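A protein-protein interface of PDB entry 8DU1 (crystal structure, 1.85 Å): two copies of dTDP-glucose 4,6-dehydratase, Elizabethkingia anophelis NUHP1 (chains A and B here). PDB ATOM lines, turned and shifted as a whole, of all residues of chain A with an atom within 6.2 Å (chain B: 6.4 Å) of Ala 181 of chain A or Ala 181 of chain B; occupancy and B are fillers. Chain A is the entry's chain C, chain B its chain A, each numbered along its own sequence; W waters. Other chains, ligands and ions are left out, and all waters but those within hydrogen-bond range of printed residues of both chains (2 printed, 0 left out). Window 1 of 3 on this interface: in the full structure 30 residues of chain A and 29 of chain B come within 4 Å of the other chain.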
ATOM      1  N   ASN A 110      -0.406 -12.751  -6.925  1.00  0.00           N
ATOM      2  CA  ASN A 110      -0.465 -11.562  -6.084  1.00  0.00           C
ATOM      3  C   ASN A 110       0.711 -10.631  -6.325  1.00  0.00           C
ATOM      4  O   ASN A 110       0.542  -9.410  -6.264  1.00  0.00           O
ATOM      5  CB  ASN A 110      -0.551 -11.959  -4.614  1.00  0.00           C
ATOM      6  CG  ASN A 110      -1.815 -12.739  -4.323  1.00  0.00           C
ATOM      7  OD1 ASN A 110      -2.669 -12.851  -5.190  1.00  0.00           O
ATOM      8  ND2 ASN A 110      -1.936 -13.278  -3.124  1.00  0.00           N
ATOM      9  N   VAL A 111       1.883 -11.174  -6.635  1.00  0.00           N
ATOM     10  CA  VAL A 111       3.074 -10.336  -6.770  1.00  0.00           C
ATOM     11  C   VAL A 111       3.405 -10.095  -8.240  1.00  0.00           C
ATOM     12  O   VAL A 111       3.435  -8.945  -8.692  1.00  0.00           O
ATOM     13  CB  VAL A 111       4.267 -10.953  -6.020  1.00  0.00           C
ATOM     14  CG1 VAL A 111       5.454 -10.009  -6.067  1.00  0.00           C
ATOM     15  CG2 VAL A 111       3.882 -11.236  -4.570  1.00  0.00           C
ATOM     16  N   VAL A 153      -1.466  -7.051   6.170  1.00  0.00           N
ATOM     17  CA  VAL A 153      -0.089  -6.600   5.975  1.00  0.00           C
ATOM     18  C   VAL A 153       0.509  -6.071   7.273  1.00  0.00           C
ATOM     19  O   VAL A 153       1.738  -6.049   7.425  1.00  0.00           O
ATOM     20  CB  VAL A 153       0.005  -5.521   4.870  1.00  0.00           C
ATOM     21  CG1 VAL A 153      -0.556  -6.026   3.525  1.00  0.00           C
ATOM     22  CG2 VAL A 153      -0.687  -4.223   5.314  1.00  0.00           C
ATOM     23  N   TYR A 169       4.607  -2.646   8.534  1.00  0.00           N
ATOM     24  CA  TYR A 169       4.215  -3.933   7.970  1.00  0.00           C
ATOM     25  C   TYR A 169       4.828  -5.070   8.767  1.00  0.00           C
ATOM     26  O   TYR A 169       5.998  -5.017   9.160  1.00  0.00           O
ATOM     27  CB  TYR A 169       4.665  -4.054   6.509  1.00  0.00           C
ATOM     28  CG  TYR A 169       3.737  -3.443   5.487  1.00  0.00           C
ATOM     29  CD1 TYR A 169       2.851  -2.425   5.836  1.00  0.00           C
ATOM     30  CD2 TYR A 169       3.751  -3.886   4.163  1.00  0.00           C
ATOM     31  CE1 TYR A 169       1.997  -1.861   4.900  1.00  0.00           C
ATOM     32  CE2 TYR A 169       2.892  -3.333   3.218  1.00  0.00           C
ATOM     33  CZ  TYR A 169       2.030  -2.314   3.599  1.00  0.00           C
ATOM     34  OH  TYR A 169       1.193  -1.755   2.679  1.00  0.00           O
ATOM     35  N   SER A 176      -0.526 -12.987   3.321  1.00  0.00           N
ATOM     36  CA  SER A 176      -0.416 -11.572   3.643  1.00  0.00           C
ATOM     37  C   SER A 176       0.973 -11.048   3.291  1.00  0.00           C
ATOM     38  O   SER A 176       1.118  -9.864   2.959  1.00  0.00           O
ATOM     39  CB  SER A 176      -0.774 -11.317   5.117  1.00  0.00           C
ATOM     40  OG  SER A 176       0.137 -11.911   6.039  1.00  0.00           O
ATOM     41  N   ALA A 177       1.991 -11.913   3.299  1.00  0.00           N
ATOM     42  CA  ALA A 177       3.297 -11.483   2.784  1.00  0.00           C
ATOM     43  C   ALA A 177       3.217 -11.166   1.292  1.00  0.00           C
ATOM     44  O   ALA A 177       3.782 -10.169   0.826  1.00  0.00           O
ATOM     45  CB  ALA A 177       4.350 -12.554   3.059  1.00  0.00           C
ATOM     46  N   SER A 178       2.477 -11.973   0.528  1.00  0.00           N
ATOM     47  CA  SER A 178       2.365 -11.700  -0.902  1.00  0.00           C
ATOM     48  C   SER A 178       1.560 -10.428  -1.156  1.00  0.00           C
ATOM     49  O   SER A 178       1.852  -9.674  -2.094  1.00  0.00           O
ATOM     50  CB  SER A 178       1.751 -12.896  -1.633  1.00  0.00           C
ATOM     51  OG  SER A 178       0.370 -13.066  -1.330  1.00  0.00           O
ATOM     52  N   LYS A 179       0.534 -10.163  -0.338  1.00  0.00           N
ATOM     53  CA  LYS A 179      -0.192  -8.905  -0.497  1.00  0.00           C
ATOM     54  C   LYS A 179       0.680  -7.722  -0.098  1.00  0.00           C
ATOM     55  O   LYS A 179       0.703  -6.700  -0.798  1.00  0.00           O
ATOM     56  CB  LYS A 179      -1.489  -8.928   0.312  1.00  0.00           C
ATOM     57  CG  LYS A 179      -2.551  -9.892  -0.229  1.00  0.00           C
ATOM     58  CD  LYS A 179      -3.081  -9.490  -1.639  1.00  0.00           C
ATOM     59  CE  LYS A 179      -3.689  -8.077  -1.659  1.00  0.00           C
ATOM     60  NZ  LYS A 179      -4.303  -7.687  -2.991  1.00  0.00           N
ATOM     61  N   ALA A 180       1.423  -7.853   1.009  1.00  0.00           N
ATOM     62  CA  ALA A 180       2.334  -6.784   1.407  1.00  0.00           C
ATOM     63  C   ALA A 180       3.332  -6.492   0.298  1.00  0.00           C
ATOM     64  O   ALA A 180       3.599  -5.328  -0.008  1.00  0.00           O
ATOM     65  CB  ALA A 180       3.054  -7.153   2.706  1.00  0.00           C
ATOM     66  N   ALA A 181       3.861  -7.545  -0.342  1.00  0.00           N
ATOM     67  CA  ALA A 181       4.761  -7.371  -1.483  1.00  0.00           C
ATOM     68  C   ALA A 181       4.116  -6.554  -2.592  1.00  0.00           C
ATOM     69  O   ALA A 181       4.766  -5.705  -3.212  1.00  0.00           O
ATOM     70  CB  ALA A 181       5.162  -8.738  -2.032  1.00  0.00           C
ATOM     71  N   SER A 182       2.845  -6.826  -2.891  1.00  0.00           N
ATOM     72  CA  SER A 182       2.208  -6.106  -3.983  1.00  0.00           C
ATOM     73  C   SER A 182       2.033  -4.633  -3.627  1.00  0.00           C
ATOM     74  O   SER A 182       2.250  -3.764  -4.480  1.00  0.00           O
ATOM     75  CB  SER A 182       0.876  -6.780  -4.355  1.00  0.00           C
ATOM     76  OG  SER A 182      -0.095  -6.614  -3.349  1.00  0.00           O
ATOM     77  N   ASP A 183       1.702  -4.335  -2.359  1.00  0.00           N
ATOM     78  CA  ASP A 183       1.651  -2.947  -1.895  1.00  0.00           C
ATOM     79  C   ASP A 183       2.976  -2.242  -2.158  1.00  0.00           C
ATOM     80  O   ASP A 183       3.007  -1.102  -2.629  1.00  0.00           O
ATOM     81  CB  ASP A 183       1.373  -2.868  -0.389  1.00  0.00           C
ATOM     82  CG  ASP A 183       0.014  -3.392   0.024  1.00  0.00           C
ATOM     83  OD1 ASP A 183      -0.710  -3.971  -0.811  1.00  0.00           O
ATOM     84  OD2 ASP A 183      -0.306  -3.204   1.217  1.00  0.00           O
ATOM     85  N   HIS A 184       4.083  -2.896  -1.789  1.00  0.00           N
ATOM     86  CA  HIS A 184       5.403  -2.296  -1.975  1.00  0.00           C
ATOM     87  C   HIS A 184       5.681  -2.004  -3.444  1.00  0.00           C
ATOM     88  O   HIS A 184       6.270  -0.968  -3.775  1.00  0.00           O
ATOM     89  CB  HIS A 184       6.503  -3.221  -1.434  1.00  0.00           C
ATOM     90  CG  HIS A 184       6.480  -3.396   0.049  1.00  0.00           C
ATOM     91  ND1 HIS A 184       6.074  -2.397   0.907  1.00  0.00           N
ATOM     92  CD2 HIS A 184       6.820  -4.451   0.825  1.00  0.00           C
ATOM     93  CE1 HIS A 184       6.153  -2.835   2.152  1.00  0.00           C
ATOM     94  NE2 HIS A 184       6.594  -4.080   2.130  1.00  0.00           N
ATOM     95  N   LEU A 185       5.340  -2.944  -4.329  1.00  0.00           N
ATOM     96  CA  LEU A 185       5.584  -2.725  -5.752  1.00  0.00           C
ATOM     97  C   LEU A 185       4.830  -1.498  -6.244  1.00  0.00           C
ATOM     98  O   LEU A 185       5.391  -0.652  -6.951  1.00  0.00           O
ATOM     99  CB  LEU A 185       5.173  -3.960  -6.558  1.00  0.00           C
ATOM    100  CG  LEU A 185       6.125  -5.162  -6.492  1.00  0.00           C
ATOM    101  CD1 LEU A 185       5.517  -6.333  -7.269  1.00  0.00           C
ATOM    102  CD2 LEU A 185       7.508  -4.802  -7.023  1.00  0.00           C
ATOM    103  N   VAL A 186       3.553  -1.380  -5.872  1.00  0.00           N
ATOM    104  CA  VAL A 186       2.760  -0.232  -6.306  1.00  0.00           C
ATOM    105  C   VAL A 186       3.409   1.066  -5.849  1.00  0.00           C
ATOM    106  O   VAL A 186       3.582   2.007  -6.636  1.00  0.00           O
ATOM    107  CB  VAL A 186       1.316  -0.344  -5.787  1.00  0.00           C
ATOM    108  CG1 VAL A 186       0.546   0.954  -6.039  1.00  0.00           C
ATOM    109  CG2 VAL A 186       0.603  -1.540  -6.420  1.00  0.00           C
ATOM    110  N   ASN B 110      14.288 -12.445  -6.714  1.00  0.00           N
ATOM    111  CA  ASN B 110      14.266 -11.975  -5.329  1.00  0.00           C
ATOM    112  C   ASN B 110      13.070 -12.495  -4.554  1.00  0.00           C
ATOM    113  O   ASN B 110      13.190 -12.748  -3.354  1.00  0.00           O
ATOM    114  CB  ASN B 110      14.295 -10.446  -5.269  1.00  0.00           C
ATOM    115  CG  ASN B 110      15.566  -9.900  -5.880  1.00  0.00           C
ATOM    116  OD1 ASN B 110      16.476 -10.674  -6.167  1.00  0.00           O
ATOM    117  ND2 ASN B 110      15.635  -8.596  -6.093  1.00  0.00           N
ATOM    118  N   VAL B 111      11.920 -12.648  -5.201  1.00  0.00           N
ATOM    119  CA  VAL B 111      10.732 -13.063  -4.464  1.00  0.00           C
ATOM    120  C   VAL B 111      10.481 -14.552  -4.675  1.00  0.00           C
ATOM    121  O   VAL B 111      10.454 -15.327  -3.716  1.00  0.00           O
ATOM    122  CB  VAL B 111       9.504 -12.241  -4.884  1.00  0.00           C
ATOM    123  CG1 VAL B 111       8.313 -12.620  -4.025  1.00  0.00           C
ATOM    124  CG2 VAL B 111       9.818 -10.753  -4.788  1.00  0.00           C
ATOM    125  N   THR B 114      13.379 -16.720  -3.443  1.00  0.00           N
ATOM    126  CA  THR B 114      13.343 -16.900  -1.994  1.00  0.00           C
ATOM    127  C   THR B 114      12.284 -17.927  -1.609  1.00  0.00           C
ATOM    128  O   THR B 114      12.542 -18.828  -0.806  1.00  0.00           O
ATOM    129  CB  THR B 114      13.084 -15.557  -1.306  1.00  0.00           C
ATOM    130  OG1 THR B 114      14.167 -14.654  -1.612  1.00  0.00           O
ATOM    131  CG2 THR B 114      13.003 -15.734   0.214  1.00  0.00           C
ATOM    132  N   HIS B 147      18.430 -14.905   6.222  1.00  0.00           N
ATOM    133  CA  HIS B 147      18.030 -14.110   5.069  1.00  0.00           C
ATOM    134  C   HIS B 147      18.789 -12.791   5.083  1.00  0.00           C
ATOM    135  O   HIS B 147      18.663 -12.017   6.034  1.00  0.00           O
ATOM    136  CB  HIS B 147      16.526 -13.848   5.098  1.00  0.00           C
ATOM    137  CG  HIS B 147      16.036 -13.058   3.931  1.00  0.00           C
ATOM    138  ND1 HIS B 147      16.105 -13.536   2.643  1.00  0.00           N
ATOM    139  CD2 HIS B 147      15.501 -11.817   3.846  1.00  0.00           C
ATOM    140  CE1 HIS B 147      15.631 -12.622   1.812  1.00  0.00           C
ATOM    141  NE2 HIS B 147      15.238 -11.580   2.519  1.00  0.00           N
ATOM    142  N   VAL B 153      14.870  -1.374   2.415  1.00  0.00           N
ATOM    143  CA  VAL B 153      13.484  -1.724   2.727  1.00  0.00           C
ATOM    144  C   VAL B 153      12.838  -0.657   3.604  1.00  0.00           C
ATOM    145  O   VAL B 153      11.608  -0.525   3.610  1.00  0.00           O
ATOM    146  CB  VAL B 153      13.367  -3.114   3.403  1.00  0.00           C
ATOM    147  CG1 VAL B 153      14.044  -4.200   2.564  1.00  0.00           C
ATOM    148  CG2 VAL B 153      13.924  -3.091   4.845  1.00  0.00           C
ATOM    149  N   TYR B 169       8.646  -0.484   7.088  1.00  0.00           N
ATOM    150  CA  TYR B 169       9.101  -0.637   5.715  1.00  0.00           C
ATOM    151  C   TYR B 169       8.474   0.433   4.841  1.00  0.00           C
ATOM    152  O   TYR B 169       7.291   0.750   4.975  1.00  0.00           O
ATOM    153  CB  TYR B 169       8.737  -2.013   5.158  1.00  0.00           C
ATOM    154  CG  TYR B 169       9.676  -3.152   5.529  1.00  0.00           C
ATOM    155  CD1 TYR B 169      10.546  -3.063   6.612  1.00  0.00           C
ATOM    156  CD2 TYR B 169       9.669  -4.323   4.789  1.00  0.00           C
ATOM    157  CE1 TYR B 169      11.402  -4.137   6.934  1.00  0.00           C
ATOM    158  CE2 TYR B 169      10.491  -5.385   5.103  1.00  0.00           C
ATOM    159  CZ  TYR B 169      11.369  -5.289   6.158  1.00  0.00           C
ATOM    160  OH  TYR B 169      12.174  -6.378   6.437  1.00  0.00           O
ATOM    161  N   SER B 176      14.146  -2.464  -4.049  1.00  0.00           N
ATOM    162  CA  SER B 176      13.993  -2.589  -2.603  1.00  0.00           C
ATOM    163  C   SER B 176      12.612  -3.128  -2.242  1.00  0.00           C
ATOM    164  O   SER B 176      12.460  -3.784  -1.204  1.00  0.00           O
ATOM    165  CB  SER B 176      14.271  -1.253  -1.907  1.00  0.00           C
ATOM    166  OG  SER B 176      13.414  -0.226  -2.359  1.00  0.00           O
ATOM    167  N   ALA B 177      11.614  -2.913  -3.110  1.00  0.00           N
ATOM    168  CA  ALA B 177      10.308  -3.533  -2.895  1.00  0.00           C
ATOM    169  C   ALA B 177      10.398  -5.055  -3.011  1.00  0.00           C
ATOM    170  O   ALA B 177       9.809  -5.783  -2.202  1.00  0.00           O
ATOM    171  CB  ALA B 177       9.302  -2.957  -3.901  1.00  0.00           C
ATOM    172  N   SER B 178      11.149  -5.557  -3.996  1.00  0.00           N
ATOM    173  CA  SER B 178      11.320  -7.003  -4.121  1.00  0.00           C
ATOM    174  C   SER B 178      12.103  -7.574  -2.939  1.00  0.00           C
ATOM    175  O   SER B 178      11.807  -8.680  -2.470  1.00  0.00           O
ATOM    176  CB  SER B 178      12.015  -7.353  -5.446  1.00  0.00           C
ATOM    177  OG  SER B 178      13.352  -6.864  -5.489  1.00  0.00           O
ATOM    178  N   LYS B 179      13.122  -6.855  -2.458  1.00  0.00           N
ATOM    179  CA  LYS B 179      13.833  -7.318  -1.268  1.00  0.00           C
ATOM    180  C   LYS B 179      12.924  -7.297  -0.040  1.00  0.00           C
ATOM    181  O   LYS B 179      12.913  -8.251   0.747  1.00  0.00           O
ATOM    182  CB  LYS B 179      15.090  -6.475  -1.032  1.00  0.00           C
ATOM    183  CG  LYS B 179      16.211  -6.748  -2.049  1.00  0.00           C
ATOM    184  CD  LYS B 179      16.767  -8.200  -1.963  1.00  0.00           C
ATOM    185  CE  LYS B 179      17.326  -8.560  -0.586  1.00  0.00           C
ATOM    186  NZ  LYS B 179      18.105  -9.863  -0.595  1.00  0.00           N
ATOM    187  N   ALA B 180      12.155  -6.220   0.141  1.00  0.00           N
ATOM    188  CA  ALA B 180      11.202  -6.181   1.251  1.00  0.00           C
ATOM    189  C   ALA B 180      10.244  -7.364   1.178  1.00  0.00           C
ATOM    190  O   ALA B 180       9.946  -7.998   2.196  1.00  0.00           O
ATOM    191  CB  ALA B 180      10.421  -4.866   1.222  1.00  0.00           C
ATOM    192  N   ALA B 181       9.772  -7.685  -0.033  1.00  0.00           N
ATOM    193  CA  ALA B 181       8.873  -8.821  -0.215  1.00  0.00           C
ATOM    194  C   ALA B 181       9.527 -10.116   0.240  1.00  0.00           C
ATOM    195  O   ALA B 181       8.870 -10.973   0.842  1.00  0.00           O
ATOM    196  CB  ALA B 181       8.462  -8.937  -1.677  1.00  0.00           C
ATOM    197  N   SER B 182      10.815 -10.293  -0.064  1.00  0.00           N
ATOM    198  CA  SER B 182      11.472 -11.523   0.349  1.00  0.00           C
ATOM    199  C   SER B 182      11.590 -11.595   1.861  1.00  0.00           C
ATOM    200  O   SER B 182      11.433 -12.678   2.434  1.00  0.00           O
ATOM    201  CB  SER B 182      12.843 -11.675  -0.336  1.00  0.00           C
ATOM    202  OG  SER B 182      13.776 -10.682   0.036  1.00  0.00           O
ATOM    203  N   ASP B 183      11.858 -10.454   2.524  1.00  0.00           N
ATOM    204  CA  ASP B 183      11.860 -10.426   3.990  1.00  0.00           C
ATOM    205  C   ASP B 183      10.525 -10.911   4.530  1.00  0.00           C
ATOM    206  O   ASP B 183      10.462 -11.689   5.491  1.00  0.00           O
ATOM    207  CB  ASP B 183      12.097  -9.011   4.541  1.00  0.00           C
ATOM    208  CG  ASP B 183      13.417  -8.387   4.138  1.00  0.00           C
ATOM    209  OD1 ASP B 183      14.199  -8.989   3.386  1.00  0.00           O
ATOM    210  OD2 ASP B 183      13.657  -7.256   4.604  1.00  0.00           O
ATOM    211  N   HIS B 184       9.435 -10.406   3.952  1.00  0.00           N
ATOM    212  CA  HIS B 184       8.116 -10.789   4.435  1.00  0.00           C
ATOM    213  C   HIS B 184       7.894 -12.290   4.291  1.00  0.00           C
ATOM    214  O   HIS B 184       7.288 -12.919   5.161  1.00  0.00           O
ATOM    215  CB  HIS B 184       7.024 -10.024   3.677  1.00  0.00           C
ATOM    216  CG  HIS B 184       7.008  -8.545   3.926  1.00  0.00           C
ATOM    217  ND1 HIS B 184       7.353  -7.976   5.139  1.00  0.00           N
ATOM    218  CD2 HIS B 184       6.677  -7.515   3.110  1.00  0.00           C
ATOM    219  CE1 HIS B 184       7.257  -6.659   5.050  1.00  0.00           C
ATOM    220  NE2 HIS B 184       6.848  -6.353   3.830  1.00  0.00           N
ATOM    221  N   LEU B 185       8.345 -12.881   3.187  1.00  0.00           N
ATOM    222  CA  LEU B 185       8.112 -14.308   2.997  1.00  0.00           C
ATOM    223  C   LEU B 185       8.844 -15.112   4.059  1.00  0.00           C
ATOM    224  O   LEU B 185       8.293 -16.057   4.626  1.00  0.00           O
ATOM    225  CB  LEU B 185       8.558 -14.753   1.600  1.00  0.00           C
ATOM    226  CG  LEU B 185       7.644 -14.344   0.436  1.00  0.00           C
ATOM    227  CD1 LEU B 185       8.322 -14.742  -0.881  1.00  0.00           C
ATOM    228  CD2 LEU B 185       6.268 -15.017   0.567  1.00  0.00           C
ATOM    229  N   VAL B 186      10.107 -14.761   4.312  1.00  0.00           N
ATOM    230  CA  VAL B 186      10.890 -15.454   5.334  1.00  0.00           C
ATOM    231  C   VAL B 186      10.183 -15.397   6.682  1.00  0.00           C
ATOM    232  O   VAL B 186       9.977 -16.425   7.344  1.00  0.00           O
ATOM    233  CB  VAL B 186      12.305 -14.857   5.415  1.00  0.00           C
ATOM    234  CG1 VAL B 186      13.073 -15.461   6.594  1.00  0.00           C
ATOM    235  CG2 VAL B 186      13.067 -15.070   4.080  1.00  0.00           C
HETATM  236  O   HOH W   1       5.506  -0.539   6.680  1.00  0.00           O
HETATM  237  O   HOH W   2       7.744  -2.924   8.458  1.00  0.00           O
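A ring nitrogen (NE2) of His 184 of chain B is in hydrogen-bond range of a ring nitrogen (NE2) of His 184 of chain A (2.8 Å).
OH of Tyr 169 of chain A lies within hydrogen-bond range of OD2 of Asp 183 of chain A (2.5 Å).
Tyr 169 of chain A touches His 184 of chain B (CB to CE1, 3.95 Å).
His 184 of chain B touches Ala 177 of chain A.
Ala 177 of chain A touches Leu 185 of chain B.
Ala 180 of chain A touches His 184 of chain B.
CB of Ala 181 of chain A touches CB of Ala 181 of chain B, at 3.3 Å.
Ala 177 of chain B touches His 184 of chain A.
Ala 180 of chain B touches His 184 of chain A (CB to CD2, 3.6 Å).
Leu 185 of chain A touches Ala 177 of chain B (N to CB, 3.99 Å).
Printed residues of chain B within 4 Å of Ala 181 of chain A: Ala 181 (3.3 Å).
Ala 181 of chain B touches just one residue of chain A: Ala 181 (3.3 Å).
Of the printed residues of chain A, Leu 185 of chain B touches Ala 177 (3.99 Å).
Of the printed residues of chain A, Ala 177 of chain B touches His 184 and Leu 185.
Of the printed residues of chain B, Ala 180 of chain A touches His 184.
Lys 179 of chain A touches none of the printed residues of chain B.
The nearest residue of chain A that does not touch Ala 181 of chain B is His 184 of chain A (4.5 Å).
Along chain A the printed residues that touch a printed residue of chain B span positions 169 to 185.
Printed residues of chain B that touch a printed residue of chain A: Ala 177, Ala 180, Ala 181, His 184 and Leu 185.
Hydrophobic or aromatic side chains of chain B within 4 Å of the printed part of chain A: Ala 177, Ala 180, Ala 181, His 184 and Leu 185.
Tyr 169 of chain A touches His 184 of chain B, but with the chains exchanged His 184 of chain A does not touch Tyr 169 of chain B (4.05 Å).
Ala 180 of chain A touches His 184 of chain B, and with the chains exchanged His 184 of chain A touches Ala 180 of chain B.
Ala 181 of chain B touches its own counterpart, Ala 181 of chain A.
His 184 of chain B touches its own counterpart, His 184 of chain A.
Of the 9 pairs that touch across the chains among the printed residues, 8 have their exchanged pair printed and touching as well.
Water W1 lies within hydrogen-bond range of O of Tyr 169 of chain B (2.8 Å) and N of Tyr 169 of chain A (2.9 Å).
Water W2 bridges the backbone carbonyl oxygen (O) of Tyr 169 of chain A and the backbone NH (N) of Tyr 169 of chain B.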
